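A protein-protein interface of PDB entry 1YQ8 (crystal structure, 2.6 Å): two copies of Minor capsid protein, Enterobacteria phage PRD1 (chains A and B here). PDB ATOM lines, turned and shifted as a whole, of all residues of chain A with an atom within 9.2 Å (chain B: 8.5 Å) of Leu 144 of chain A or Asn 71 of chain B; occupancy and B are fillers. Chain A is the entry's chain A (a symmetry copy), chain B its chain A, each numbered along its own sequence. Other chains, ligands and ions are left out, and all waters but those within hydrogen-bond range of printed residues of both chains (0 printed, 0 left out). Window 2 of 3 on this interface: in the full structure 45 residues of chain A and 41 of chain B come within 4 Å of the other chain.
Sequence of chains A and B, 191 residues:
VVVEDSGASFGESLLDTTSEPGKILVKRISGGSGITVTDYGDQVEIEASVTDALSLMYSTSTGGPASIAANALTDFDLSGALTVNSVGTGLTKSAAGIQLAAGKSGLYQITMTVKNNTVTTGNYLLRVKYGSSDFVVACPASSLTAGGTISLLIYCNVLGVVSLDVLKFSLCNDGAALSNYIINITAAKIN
OD2 of Asp 134 of chain B lies within salt-bridge range of NZ of Lys 115 of chain A (3.8 Å).
Of the 25 printed residues of chain B, 7 touch a printed residue of chain A. Hydrophobic or aromatic side chains of chain A within 4 Å of the printed part of chain B: Pro 140 and Leu 144. Along chain A the printed residues that touch a printed residue of chain B span positions 115 to 148. Among the printed residues, 12 pairs touch across the chains.
O of Asn 173 of chain B lies within hydrogen-bond range of N of Asn 71 of chain B, 2.7 Å away. The side-chain amide nitrogen of Asn 71 of chain B lies within hydrogen-bond range of the backbone carbonyl oxygen of Asp 174 of chain B (2.8 Å). The backbone carbonyl oxygen (O) of Ala 72 of chain B sits at hydrogen-bond distance from the side-chain sulfur (SG) of Cys 172 of chain B (3.2 Å). The backbone NH (N) of Leu 125 of chain B sits at hydrogen-bond distance from the backbone carbonyl oxygen (O) of Cys 172 of chain B, at 2.7 Å. The side-chain amide oxygen (OD1) of Asn 117 of chain A sits at hydrogen-bond distance from the side-chain amino group (NZ) of Lys 115 of chain A (2.7 Å). The side-chain hydroxyl (OG1) of Thr 145 of chain A is in hydrogen-bond range of the side-chain hydroxyl (OG) of Ser 142 of chain A (2.5 Å).
Among the printed residues, merely in contact across the chains: Pro 140 of chain A with Ala 138 of chain B, Leu 144 of chain A with Asn 71 of chain B, Gly 147 of chain A with Val 136 of chain B, Gly 148 of chain A with Val 136 of chain B, Thr 145 of chain A with Leu 125 of chain B, Leu 144 of chain A with Ala 72 of chain B, Leu 144 of chain A with Leu 73 of chain B, Thr 145 of chain A with Val 136 of chain B, Leu 144 of chain A with Leu 125 of chain B, Thr 145 of chain A with Ala 138 of chain B and Lys 115 of chain A with Val 136 of chain B.
No position is printed for both chains.
Of chain B, only Asn 71 (3.2 Å), Ala 72 (3.7 Å), Leu 73 (3.7 Å) and Leu 125 (3.8 Å) come within 4 Å of Leu 144 of chain A. Of chain A, only Leu 144 (3.2 Å) comes within 4 Å of Asn 71 of chain B. No residue of chain A comes within 4 Å of Ala 70 of chain B. Of the printed residues of chain A, Leu 73 of chain B touches Leu 144 (3.7 Å). Of the printed residues of chain B, Pro 140 of chain A touches Ala 138 (3.0 Å). Printed residues of chain B within 4 Å of Thr 145 of chain A: Leu 125 (3.6 Å), Val 136 (3.8 Å) and Ala 138 (3.8 Å). The nearest residue of chain A that does not touch Asn 71 of chain B is Ser 142 of chain A (6.7 Å).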
ATOM      1  N   VAL A 114     -13.287  -4.017  19.625  1.00  0.00           N
ATOM      2  CA  VAL A 114     -13.483  -4.772  20.849  1.00  0.00           C
ATOM      3  C   VAL A 114     -12.188  -4.794  21.642  1.00  0.00           C
ATOM      4  O   VAL A 114     -11.101  -4.621  21.097  1.00  0.00           O
ATOM      5  CB  VAL A 114     -13.965  -6.215  20.586  1.00  0.00           C
ATOM      6  CG1 VAL A 114     -12.862  -7.056  20.000  1.00  0.00           C
ATOM      7  CG2 VAL A 114     -14.450  -6.819  21.872  1.00  0.00           C
ATOM      8  N   LYS A 115     -12.321  -4.968  22.944  1.00  0.00           N
ATOM      9  CA  LYS A 115     -11.190  -5.018  23.846  1.00  0.00           C
ATOM     10  C   LYS A 115     -11.671  -5.831  25.024  1.00  0.00           C
ATOM     11  O   LYS A 115     -12.654  -5.470  25.670  1.00  0.00           O
ATOM     12  CB  LYS A 115     -10.804  -3.611  24.312  1.00  0.00           C
ATOM     13  CG  LYS A 115      -9.737  -2.929  23.451  1.00  0.00           C
ATOM     14  CD  LYS A 115      -8.432  -3.697  23.505  1.00  0.00           C
ATOM     15  CE  LYS A 115      -7.914  -3.798  24.928  1.00  0.00           C
ATOM     16  NZ  LYS A 115      -6.700  -4.655  24.995  1.00  0.00           N
ATOM     17  N   ASN A 117      -9.365  -7.458  27.675  1.00  0.00           N
ATOM     18  CA  ASN A 117      -8.087  -7.776  28.281  1.00  0.00           C
ATOM     19  C   ASN A 117      -7.853  -9.187  28.815  1.00  0.00           C
ATOM     20  O   ASN A 117      -6.847  -9.811  28.487  1.00  0.00           O
ATOM     21  CB  ASN A 117      -7.790  -6.747  29.374  1.00  0.00           C
ATOM     22  CG  ASN A 117      -7.349  -5.403  28.800  1.00  0.00           C
ATOM     23  OD1 ASN A 117      -7.436  -5.175  27.591  1.00  0.00           O
ATOM     24  ND2 ASN A 117      -6.877  -4.507  29.667  1.00  0.00           N
ATOM     25  N   VAL A 119      -8.710 -11.970  27.945  1.00  0.00           N
ATOM     26  CA  VAL A 119      -8.606 -13.037  26.949  1.00  0.00           C
ATOM     27  C   VAL A 119      -7.636 -12.620  25.856  1.00  0.00           C
ATOM     28  O   VAL A 119      -7.980 -11.845  24.966  1.00  0.00           O
ATOM     29  CB  VAL A 119      -9.977 -13.367  26.331  1.00  0.00           C
ATOM     30  CG1 VAL A 119      -9.824 -14.408  25.236  1.00  0.00           C
ATOM     31  CG2 VAL A 119     -10.903 -13.891  27.408  1.00  0.00           C
ATOM     32  N   THR A 120      -6.422 -13.159  25.931  1.00  0.00           N
ATOM     33  CA  THR A 120      -5.346 -12.825  25.006  1.00  0.00           C
ATOM     34  C   THR A 120      -4.933 -13.954  24.071  1.00  0.00           C
ATOM     35  O   THR A 120      -3.879 -13.890  23.445  1.00  0.00           O
ATOM     36  CB  THR A 120      -4.103 -12.370  25.807  1.00  0.00           C
ATOM     37  OG1 THR A 120      -3.503 -13.496  26.456  1.00  0.00           O
ATOM     38  CG2 THR A 120      -4.514 -11.385  26.883  1.00  0.00           C
ATOM     39  N   THR A 121      -5.762 -14.984  23.965  1.00  0.00           N
ATOM     40  CA  THR A 121      -5.424 -16.114  23.105  1.00  0.00           C
ATOM     41  C   THR A 121      -6.461 -16.346  22.017  1.00  0.00           C
ATOM     42  O   THR A 121      -7.585 -15.862  22.109  1.00  0.00           O
ATOM     43  CB  THR A 121      -5.298 -17.411  23.921  1.00  0.00           C
ATOM     44  OG1 THR A 121      -6.568 -17.731  24.501  1.00  0.00           O
ATOM     45  CG2 THR A 121      -4.271 -17.249  25.023  1.00  0.00           C
ATOM     46  N   PRO A 140      -5.930 -11.985  15.411  1.00  0.00           N
ATOM     47  CA  PRO A 140      -5.114 -12.784  16.329  1.00  0.00           C
ATOM     48  C   PRO A 140      -4.886 -12.052  17.652  1.00  0.00           C
ATOM     49  O   PRO A 140      -4.494 -10.885  17.675  1.00  0.00           O
ATOM     50  CB  PRO A 140      -3.827 -12.986  15.546  1.00  0.00           C
ATOM     51  CG  PRO A 140      -4.294 -13.007  14.144  1.00  0.00           C
ATOM     52  CD  PRO A 140      -5.285 -11.882  14.094  1.00  0.00           C
ATOM     53  N   ALA A 141      -5.131 -12.745  18.757  1.00  0.00           N
ATOM     54  CA  ALA A 141      -4.971 -12.141  20.083  1.00  0.00           C
ATOM     55  C   ALA A 141      -3.543 -12.063  20.607  1.00  0.00           C
ATOM     56  O   ALA A 141      -2.580 -12.277  19.885  1.00  0.00           O
ATOM     57  CB  ALA A 141      -5.838 -12.879  21.089  1.00  0.00           C
ATOM     58  N   SER A 142      -3.435 -11.745  21.888  1.00  0.00           N
ATOM     59  CA  SER A 142      -2.159 -11.614  22.594  1.00  0.00           C
ATOM     60  C   SER A 142      -2.453 -10.614  23.679  1.00  0.00           C
ATOM     61  O   SER A 142      -3.430  -9.883  23.571  1.00  0.00           O
ATOM     62  CB  SER A 142      -1.056 -11.065  21.683  1.00  0.00           C
ATOM     63  OG  SER A 142      -1.357  -9.762  21.216  1.00  0.00           O
ATOM     64  N   SER A 143      -1.638 -10.585  24.728  1.00  0.00           N
ATOM     65  CA  SER A 143      -1.872  -9.634  25.798  1.00  0.00           C
ATOM     66  C   SER A 143      -1.735  -8.205  25.270  1.00  0.00           C
ATOM     67  O   SER A 143      -2.478  -7.317  25.679  1.00  0.00           O
ATOM     68  CB  SER A 143      -0.895  -9.868  26.954  1.00  0.00           C
ATOM     69  OG  SER A 143      -1.205 -11.060  27.655  1.00  0.00           O
ATOM     70  N   LEU A 144      -0.792  -7.989  24.356  1.00  0.00           N
ATOM     71  CA  LEU A 144      -0.590  -6.663  23.767  1.00  0.00           C
ATOM     72  C   LEU A 144      -1.763  -6.232  22.869  1.00  0.00           C
ATOM     73  O   LEU A 144      -2.095  -5.049  22.796  1.00  0.00           O
ATOM     74  CB  LEU A 144       0.713  -6.639  22.972  1.00  0.00           C
ATOM     75  CG  LEU A 144       1.964  -6.487  23.837  1.00  0.00           C
ATOM     76  CD1 LEU A 144       3.224  -6.747  23.024  1.00  0.00           C
ATOM     77  CD2 LEU A 144       1.981  -5.092  24.411  1.00  0.00           C
ATOM     78  N   THR A 145      -2.380  -7.196  22.185  1.00  0.00           N
ATOM     79  CA  THR A 145      -3.520  -6.925  21.318  1.00  0.00           C
ATOM     80  C   THR A 145      -4.640  -7.868  21.726  1.00  0.00           C
ATOM     81  O   THR A 145      -4.954  -8.832  21.028  1.00  0.00           O
ATOM     82  CB  THR A 145      -3.171  -7.125  19.806  1.00  0.00           C
ATOM     83  OG1 THR A 145      -2.680  -8.451  19.577  1.00  0.00           O
ATOM     84  CG2 THR A 145      -2.101  -6.145  19.378  1.00  0.00           C
ATOM     85  N   ALA A 146      -5.228  -7.590  22.883  1.00  0.00           N
ATOM     86  CA  ALA A 146      -6.318  -8.396  23.403  1.00  0.00           C
ATOM     87  C   ALA A 146      -7.637  -7.840  22.898  1.00  0.00           C
ATOM     88  O   ALA A 146      -8.490  -7.427  23.681  1.00  0.00           O
ATOM     89  CB  ALA A 146      -6.293  -8.389  24.914  1.00  0.00           C
ATOM     90  N   GLY A 147      -7.797  -7.826  21.579  1.00  0.00           N
ATOM     91  CA  GLY A 147      -9.019  -7.306  20.993  1.00  0.00           C
ATOM     92  C   GLY A 147      -9.052  -7.428  19.484  1.00  0.00           C
ATOM     93  O   GLY A 147      -8.291  -8.190  18.903  1.00  0.00           O
ATOM     94  N   GLY A 148      -9.934  -6.662  18.852  1.00  0.00           N
ATOM     95  CA  GLY A 148     -10.062  -6.711  17.411  1.00  0.00           C
ATOM     96  C   GLY A 148     -10.755  -5.477  16.878  1.00  0.00           C
ATOM     97  O   GLY A 148     -11.356  -4.718  17.630  1.00  0.00           O
ATOM     98  N   ILE B  68      12.303  -0.369  16.026  1.00  0.00           N
ATOM     99  CA  ILE B  68      11.082  -0.570  16.793  1.00  0.00           C
ATOM    100  C   ILE B  68      11.340  -1.917  17.467  1.00  0.00           C
ATOM    101  O   ILE B  68      11.417  -2.936  16.794  1.00  0.00           O
ATOM    102  CB  ILE B  68       9.842  -0.677  15.871  1.00  0.00           C
ATOM    103  CG1 ILE B  68       9.739   0.535  14.956  1.00  0.00           C
ATOM    104  CG2 ILE B  68       8.584  -0.765  16.706  1.00  0.00           C
ATOM    105  CD1 ILE B  68       9.146   1.724  15.603  1.00  0.00           C
ATOM    106  N   ALA B  69      11.494  -1.910  18.785  1.00  0.00           N
ATOM    107  CA  ALA B  69      11.775  -3.127  19.541  1.00  0.00           C
ATOM    108  C   ALA B  69      10.728  -4.225  19.375  1.00  0.00           C
ATOM    109  O   ALA B  69       9.527  -3.967  19.428  1.00  0.00           O
ATOM    110  CB  ALA B  69      11.942  -2.784  21.013  1.00  0.00           C
ATOM    111  N   ALA B  70      11.195  -5.457  19.188  1.00  0.00           N
ATOM    112  CA  ALA B  70      10.296  -6.593  19.000  1.00  0.00           C
ATOM    113  C   ALA B  70       9.299  -6.749  20.132  1.00  0.00           C
ATOM    114  O   ALA B  70       9.496  -6.227  21.231  1.00  0.00           O
ATOM    115  CB  ALA B  70      11.092  -7.880  18.836  1.00  0.00           C
ATOM    116  N   ASN B  71       8.224  -7.466  19.829  1.00  0.00           N
ATOM    117  CA  ASN B  71       7.141  -7.756  20.763  1.00  0.00           C
ATOM    118  C   ASN B  71       6.960  -6.802  21.939  1.00  0.00           C
ATOM    119  O   ASN B  71       7.274  -7.145  23.068  1.00  0.00           O
ATOM    120  CB  ASN B  71       7.302  -9.172  21.301  1.00  0.00           C
ATOM    121  CG  ASN B  71       6.008  -9.732  21.821  1.00  0.00           C
ATOM    122  OD1 ASN B  71       5.314  -9.085  22.603  1.00  0.00           O
ATOM    123  ND2 ASN B  71       5.665 -10.941  21.384  1.00  0.00           N
ATOM    124  N   ALA B  72       6.427  -5.616  21.670  1.00  0.00           N
ATOM    125  CA  ALA B  72       6.198  -4.604  22.699  1.00  0.00           C
ATOM    126  C   ALA B  72       5.712  -3.307  22.046  1.00  0.00           C
ATOM    127  O   ALA B  72       6.142  -2.962  20.947  1.00  0.00           O
ATOM    128  CB  ALA B  72       7.486  -4.353  23.495  1.00  0.00           C
ATOM    129  N   LEU B  73       4.827  -2.579  22.719  1.00  0.00           N
ATOM    130  CA  LEU B  73       4.303  -1.340  22.150  1.00  0.00           C
ATOM    131  C   LEU B  73       4.602  -0.111  23.010  1.00  0.00           C
ATOM    132  O   LEU B  73       4.124  -0.002  24.129  1.00  0.00           O
ATOM    133  CB  LEU B  73       2.790  -1.477  21.940  1.00  0.00           C
ATOM    134  CG  LEU B  73       2.335  -2.717  21.160  1.00  0.00           C
ATOM    135  CD1 LEU B  73       0.904  -3.035  21.523  1.00  0.00           C
ATOM    136  CD2 LEU B  73       2.476  -2.500  19.671  1.00  0.00           C
ATOM    137  N   THR B  74       5.410   0.799  22.473  1.00  0.00           N
ATOM    138  CA  THR B  74       5.793   2.047  23.138  1.00  0.00           C
ATOM    139  C   THR B  74       5.214   3.184  22.298  1.00  0.00           C
ATOM    140  O   THR B  74       5.578   3.325  21.137  1.00  0.00           O
ATOM    141  CB  THR B  74       7.311   2.221  23.148  1.00  0.00           C
ATOM    142  OG1 THR B  74       7.940   0.985  23.502  1.00  0.00           O
ATOM    143  CG2 THR B  74       7.711   3.284  24.144  1.00  0.00           C
ATOM    144  N   ASN B 123       3.331 -11.866  13.798  1.00  0.00           N
ATOM    145  CA  ASN B 123       2.234 -10.943  13.532  1.00  0.00           C
ATOM    146  C   ASN B 123       2.633  -9.495  13.809  1.00  0.00           C
ATOM    147  O   ASN B 123       3.505  -9.220  14.643  1.00  0.00           O
ATOM    148  CB  ASN B 123       1.022 -11.286  14.384  1.00  0.00           C
ATOM    149  CG  ASN B 123       0.564 -12.710  14.192  1.00  0.00           C
ATOM    150  OD1 ASN B 123       0.410 -13.181  13.064  1.00  0.00           O
ATOM    151  ND2 ASN B 123       0.328 -13.407  15.299  1.00  0.00           N
ATOM    152  N   LEU B 125       1.640  -6.119  15.383  1.00  0.00           N
ATOM    153  CA  LEU B 125       0.727  -5.633  16.405  1.00  0.00           C
ATOM    154  C   LEU B 125       0.564  -4.136  16.223  1.00  0.00           C
ATOM    155  O   LEU B 125       1.554  -3.415  16.178  1.00  0.00           O
ATOM    156  CB  LEU B 125       1.301  -5.921  17.790  1.00  0.00           C
ATOM    157  CG  LEU B 125       1.747  -7.361  18.037  1.00  0.00           C
ATOM    158  CD1 LEU B 125       2.398  -7.456  19.401  1.00  0.00           C
ATOM    159  CD2 LEU B 125       0.557  -8.296  17.929  1.00  0.00           C
ATOM    160  N   LEU B 126      -0.676  -3.668  16.110  1.00  0.00           N
ATOM    161  CA  LEU B 126      -0.943  -2.241  15.932  1.00  0.00           C
ATOM    162  C   LEU B 126      -1.842  -1.675  17.037  1.00  0.00           C
ATOM    163  O   LEU B 126      -2.717  -2.365  17.569  1.00  0.00           O
ATOM    164  CB  LEU B 126      -1.572  -1.995  14.560  1.00  0.00           C
ATOM    165  CG  LEU B 126      -0.704  -2.363  13.352  1.00  0.00           C
ATOM    166  CD1 LEU B 126      -0.580  -3.862  13.206  1.00  0.00           C
ATOM    167  CD2 LEU B 126      -1.338  -1.781  12.114  1.00  0.00           C
ATOM    168  N   ARG B 127      -1.636  -0.409  17.378  1.00  0.00           N
ATOM    169  CA  ARG B 127      -2.420   0.186  18.439  1.00  0.00           C
ATOM    170  C   ARG B 127      -2.556   1.703  18.452  1.00  0.00           C
ATOM    171  O   ARG B 127      -1.580   2.448  18.474  1.00  0.00           O
ATOM    172  CB  ARG B 127      -1.859  -0.259  19.774  1.00  0.00           C
ATOM    173  CG  ARG B 127      -2.776   0.026  20.919  1.00  0.00           C
ATOM    174  CD  ARG B 127      -2.131  -0.429  22.176  1.00  0.00           C
ATOM    175  NE  ARG B 127      -1.058   0.468  22.555  1.00  0.00           N
ATOM    176  CZ  ARG B 127      -0.213   0.224  23.547  1.00  0.00           C
ATOM    177  NH1 ARG B 127      -0.325  -0.899  24.239  1.00  0.00           N
ATOM    178  NH2 ARG B 127       0.720   1.112  23.860  1.00  0.00           N
ATOM    179  N   ASP B 134      -8.593   2.226  24.115  1.00  0.00           N
ATOM    180  CA  ASP B 134      -7.508   1.888  23.204  1.00  0.00           C
ATOM    181  C   ASP B 134      -7.946   0.791  22.247  1.00  0.00           C
ATOM    182  O   ASP B 134      -8.557  -0.202  22.657  1.00  0.00           O
ATOM    183  CB  ASP B 134      -6.266   1.434  23.973  1.00  0.00           C
ATOM    184  CG  ASP B 134      -6.551   0.309  24.935  1.00  0.00           C
ATOM    185  OD1 ASP B 134      -6.877   0.603  26.109  1.00  0.00           O
ATOM    186  OD2 ASP B 134      -6.448  -0.866  24.518  1.00  0.00           O
ATOM    187  N   PHE B 135      -7.620   0.970  20.972  1.00  0.00           N
ATOM    188  CA  PHE B 135      -8.010   0.022  19.937  1.00  0.00           C
ATOM    189  C   PHE B 135      -6.827  -0.753  19.355  1.00  0.00           C
ATOM    190  O   PHE B 135      -5.773  -0.176  19.066  1.00  0.00           O
ATOM    191  CB  PHE B 135      -8.775   0.782  18.852  1.00  0.00           C
ATOM    192  CG  PHE B 135      -9.757   1.780  19.408  1.00  0.00           C
ATOM    193  CD1 PHE B 135      -9.365   3.092  19.670  1.00  0.00           C
ATOM    194  CD2 PHE B 135     -11.061   1.399  19.721  1.00  0.00           C
ATOM    195  CE1 PHE B 135     -10.253   4.013  20.241  1.00  0.00           C
ATOM    196  CE2 PHE B 135     -11.952   2.307  20.291  1.00  0.00           C
ATOM    197  CZ  PHE B 135     -11.546   3.616  20.551  1.00  0.00           C
ATOM    198  N   VAL B 136      -7.011  -2.061  19.181  1.00  0.00           N
ATOM    199  CA  VAL B 136      -5.946  -2.917  18.669  1.00  0.00           C
ATOM    200  C   VAL B 136      -6.303  -3.860  17.505  1.00  0.00           C
ATOM    201  O   VAL B 136      -7.464  -4.007  17.128  1.00  0.00           O
ATOM    202  CB  VAL B 136      -5.380  -3.771  19.809  1.00  0.00           C
ATOM    203  CG1 VAL B 136      -4.957  -2.875  20.961  1.00  0.00           C
ATOM    204  CG2 VAL B 136      -6.427  -4.779  20.268  1.00  0.00           C
ATOM    205  N   VAL B 137      -5.271  -4.488  16.947  1.00  0.00           N
ATOM    206  CA  VAL B 137      -5.416  -5.446  15.853  1.00  0.00           C
ATOM    207  C   VAL B 137      -4.063  -6.071  15.507  1.00  0.00           C
ATOM    208  O   VAL B 137      -3.051  -5.379  15.405  1.00  0.00           O
ATOM    209  CB  VAL B 137      -6.034  -4.783  14.568  1.00  0.00           C
ATOM    210  CG1 VAL B 137      -5.013  -3.872  13.894  1.00  0.00           C
ATOM    211  CG2 VAL B 137      -6.545  -5.861  13.599  1.00  0.00           C
ATOM    212  N   ALA B 138      -4.054  -7.392  15.356  1.00  0.00           N
ATOM    213  CA  ALA B 138      -2.835  -8.115  15.013  1.00  0.00           C
ATOM    214  C   ALA B 138      -2.891  -8.517  13.544  1.00  0.00           C
ATOM    215  O   ALA B 138      -3.902  -9.025  13.059  1.00  0.00           O
ATOM    216  CB  ALA B 138      -2.691  -9.347  15.886  1.00  0.00           C
ATOM    217  N   SER B 170       1.102   3.381  18.095  1.00  0.00           N
ATOM    218  CA  SER B 170       2.130   2.376  18.358  1.00  0.00           C
ATOM    219  C   SER B 170       1.934   1.053  17.621  1.00  0.00           C
ATOM    220  O   SER B 170       0.819   0.571  17.478  1.00  0.00           O
ATOM    221  CB  SER B 170       2.225   2.122  19.867  1.00  0.00           C
ATOM    222  OG  SER B 170       3.216   1.157  20.163  1.00  0.00           O
ATOM    223  N   LEU B 171       3.030   0.476  17.144  1.00  0.00           N
ATOM    224  CA  LEU B 171       2.985  -0.794  16.434  1.00  0.00           C
ATOM    225  C   LEU B 171       4.343  -1.487  16.520  1.00  0.00           C
ATOM    226  O   LEU B 171       5.338  -0.867  16.914  1.00  0.00           O
ATOM    227  CB  LEU B 171       2.594  -0.582  14.960  1.00  0.00           C
ATOM    228  CG  LEU B 171       3.454   0.219  13.964  1.00  0.00           C
ATOM    229  CD1 LEU B 171       4.755  -0.503  13.654  1.00  0.00           C
ATOM    230  CD2 LEU B 171       2.663   0.423  12.670  1.00  0.00           C
ATOM    231  N   CYS B 172       4.373  -2.767  16.139  1.00  0.00           N
ATOM    232  CA  CYS B 172       5.595  -3.575  16.156  1.00  0.00           C
ATOM    233  C   CYS B 172       5.264  -4.967  15.625  1.00  0.00           C
ATOM    234  O   CYS B 172       4.131  -5.228  15.219  1.00  0.00           O
ATOM    235  CB  CYS B 172       6.105  -3.727  17.588  1.00  0.00           C
ATOM    236  SG  CYS B 172       5.095  -4.875  18.567  1.00  0.00           S
ATOM    237  N   ASN B 173       6.263  -5.852  15.632  1.00  0.00           N
ATOM    238  CA  ASN B 173       6.096  -7.247  15.204  1.00  0.00           C
ATOM    239  C   ASN B 173       6.258  -8.029  16.501  1.00  0.00           C
ATOM    240  O   ASN B 173       7.053  -7.638  17.357  1.00  0.00           O
ATOM    241  CB  ASN B 173       7.199  -7.662  14.218  1.00  0.00           C
ATOM    242  CG  ASN B 173       6.967  -9.046  13.626  1.00  0.00           C
ATOM    243  OD1 ASN B 173       6.266  -9.191  12.634  1.00  0.00           O
ATOM    244  ND2 ASN B 173       7.543 -10.065  14.245  1.00  0.00           N
ATOM    245  N   ASP B 174       5.527  -9.124  16.670  1.00  0.00           N
ATOM    246  CA  ASP B 174       5.664  -9.864  17.918  1.00  0.00           C
ATOM    247  C   ASP B 174       6.919 -10.732  18.015  1.00  0.00           C
ATOM    248  O   ASP B 174       7.224 -11.267  19.081  1.00  0.00           O
ATOM    249  CB  ASP B 174       4.406 -10.713  18.201  1.00  0.00           C
ATOM    250  CG  ASP B 174       4.071 -11.684  17.083  1.00  0.00           C
ATOM    251  OD1 ASP B 174       4.880 -11.837  16.153  1.00  0.00           O
ATOM    252  OD2 ASP B 174       2.986 -12.304  17.149  1.00  0.00           O
ATOM    253  N   GLY B 175       7.667 -10.848  16.921  1.00  0.00           N
ATOM    254  CA  GLY B 175       8.855 -11.684  16.958  1.00  0.00           C
ATOM    255  C   GLY B 175      10.097 -11.194  16.246  1.00  0.00           C
ATOM    256  O   GLY B 175      10.934 -12.008  15.867  1.00  0.00           O
ATOM    257  N   ALA B 176      10.224  -9.878  16.070  1.00  0.00           N
ATOM    258  CA  ALA B 176      11.382  -9.281  15.413  1.00  0.00           C
ATOM    259  C   ALA B 176      11.311  -7.768  15.524  1.00  0.00           C
ATOM    260  O   ALA B 176      10.240  -7.215  15.709  1.00  0.00           O
ATOM    261  CB  ALA B 176      11.425  -9.688  13.952  1.00  0.00           C
ATOM    262  N   ALA B 177      12.453  -7.101  15.400  1.00  0.00           N
ATOM    263  CA  ALA B 177      12.504  -5.647  15.491  1.00  0.00           C
ATOM    264  C   ALA B 177      12.345  -5.021  14.117  1.00  0.00           C
ATOM    265  O   ALA B 177      12.758  -5.614  13.123  1.00  0.00           O
ATOM    266  CB  ALA B 177      13.823  -5.214  16.098  1.00  0.00           C
ATOM    267  N   LEU B 178      11.756  -3.823  14.063  1.00  0.00           N
ATOM    268  CA  LEU B 178      11.553  -3.109  12.795  1.00  0.00           C
ATOM    269  C   LEU B 178      12.508  -1.918  12.667  1.00  0.00           C
ATOM    270  O   LEU B 178      12.436  -0.956  13.436  1.00  0.00           O
ATOM    271  CB  LEU B 178      10.115  -2.594  12.687  1.00  0.00           C
ATOM    272  CG  LEU B 178       8.965  -3.527  13.054  1.00  0.00           C
ATOM    273  CD1 LEU B 178       7.666  -2.803  12.801  1.00  0.00           C
ATOM    274  CD2 LEU B 178       9.030  -4.810  12.244  1.00  0.00           C
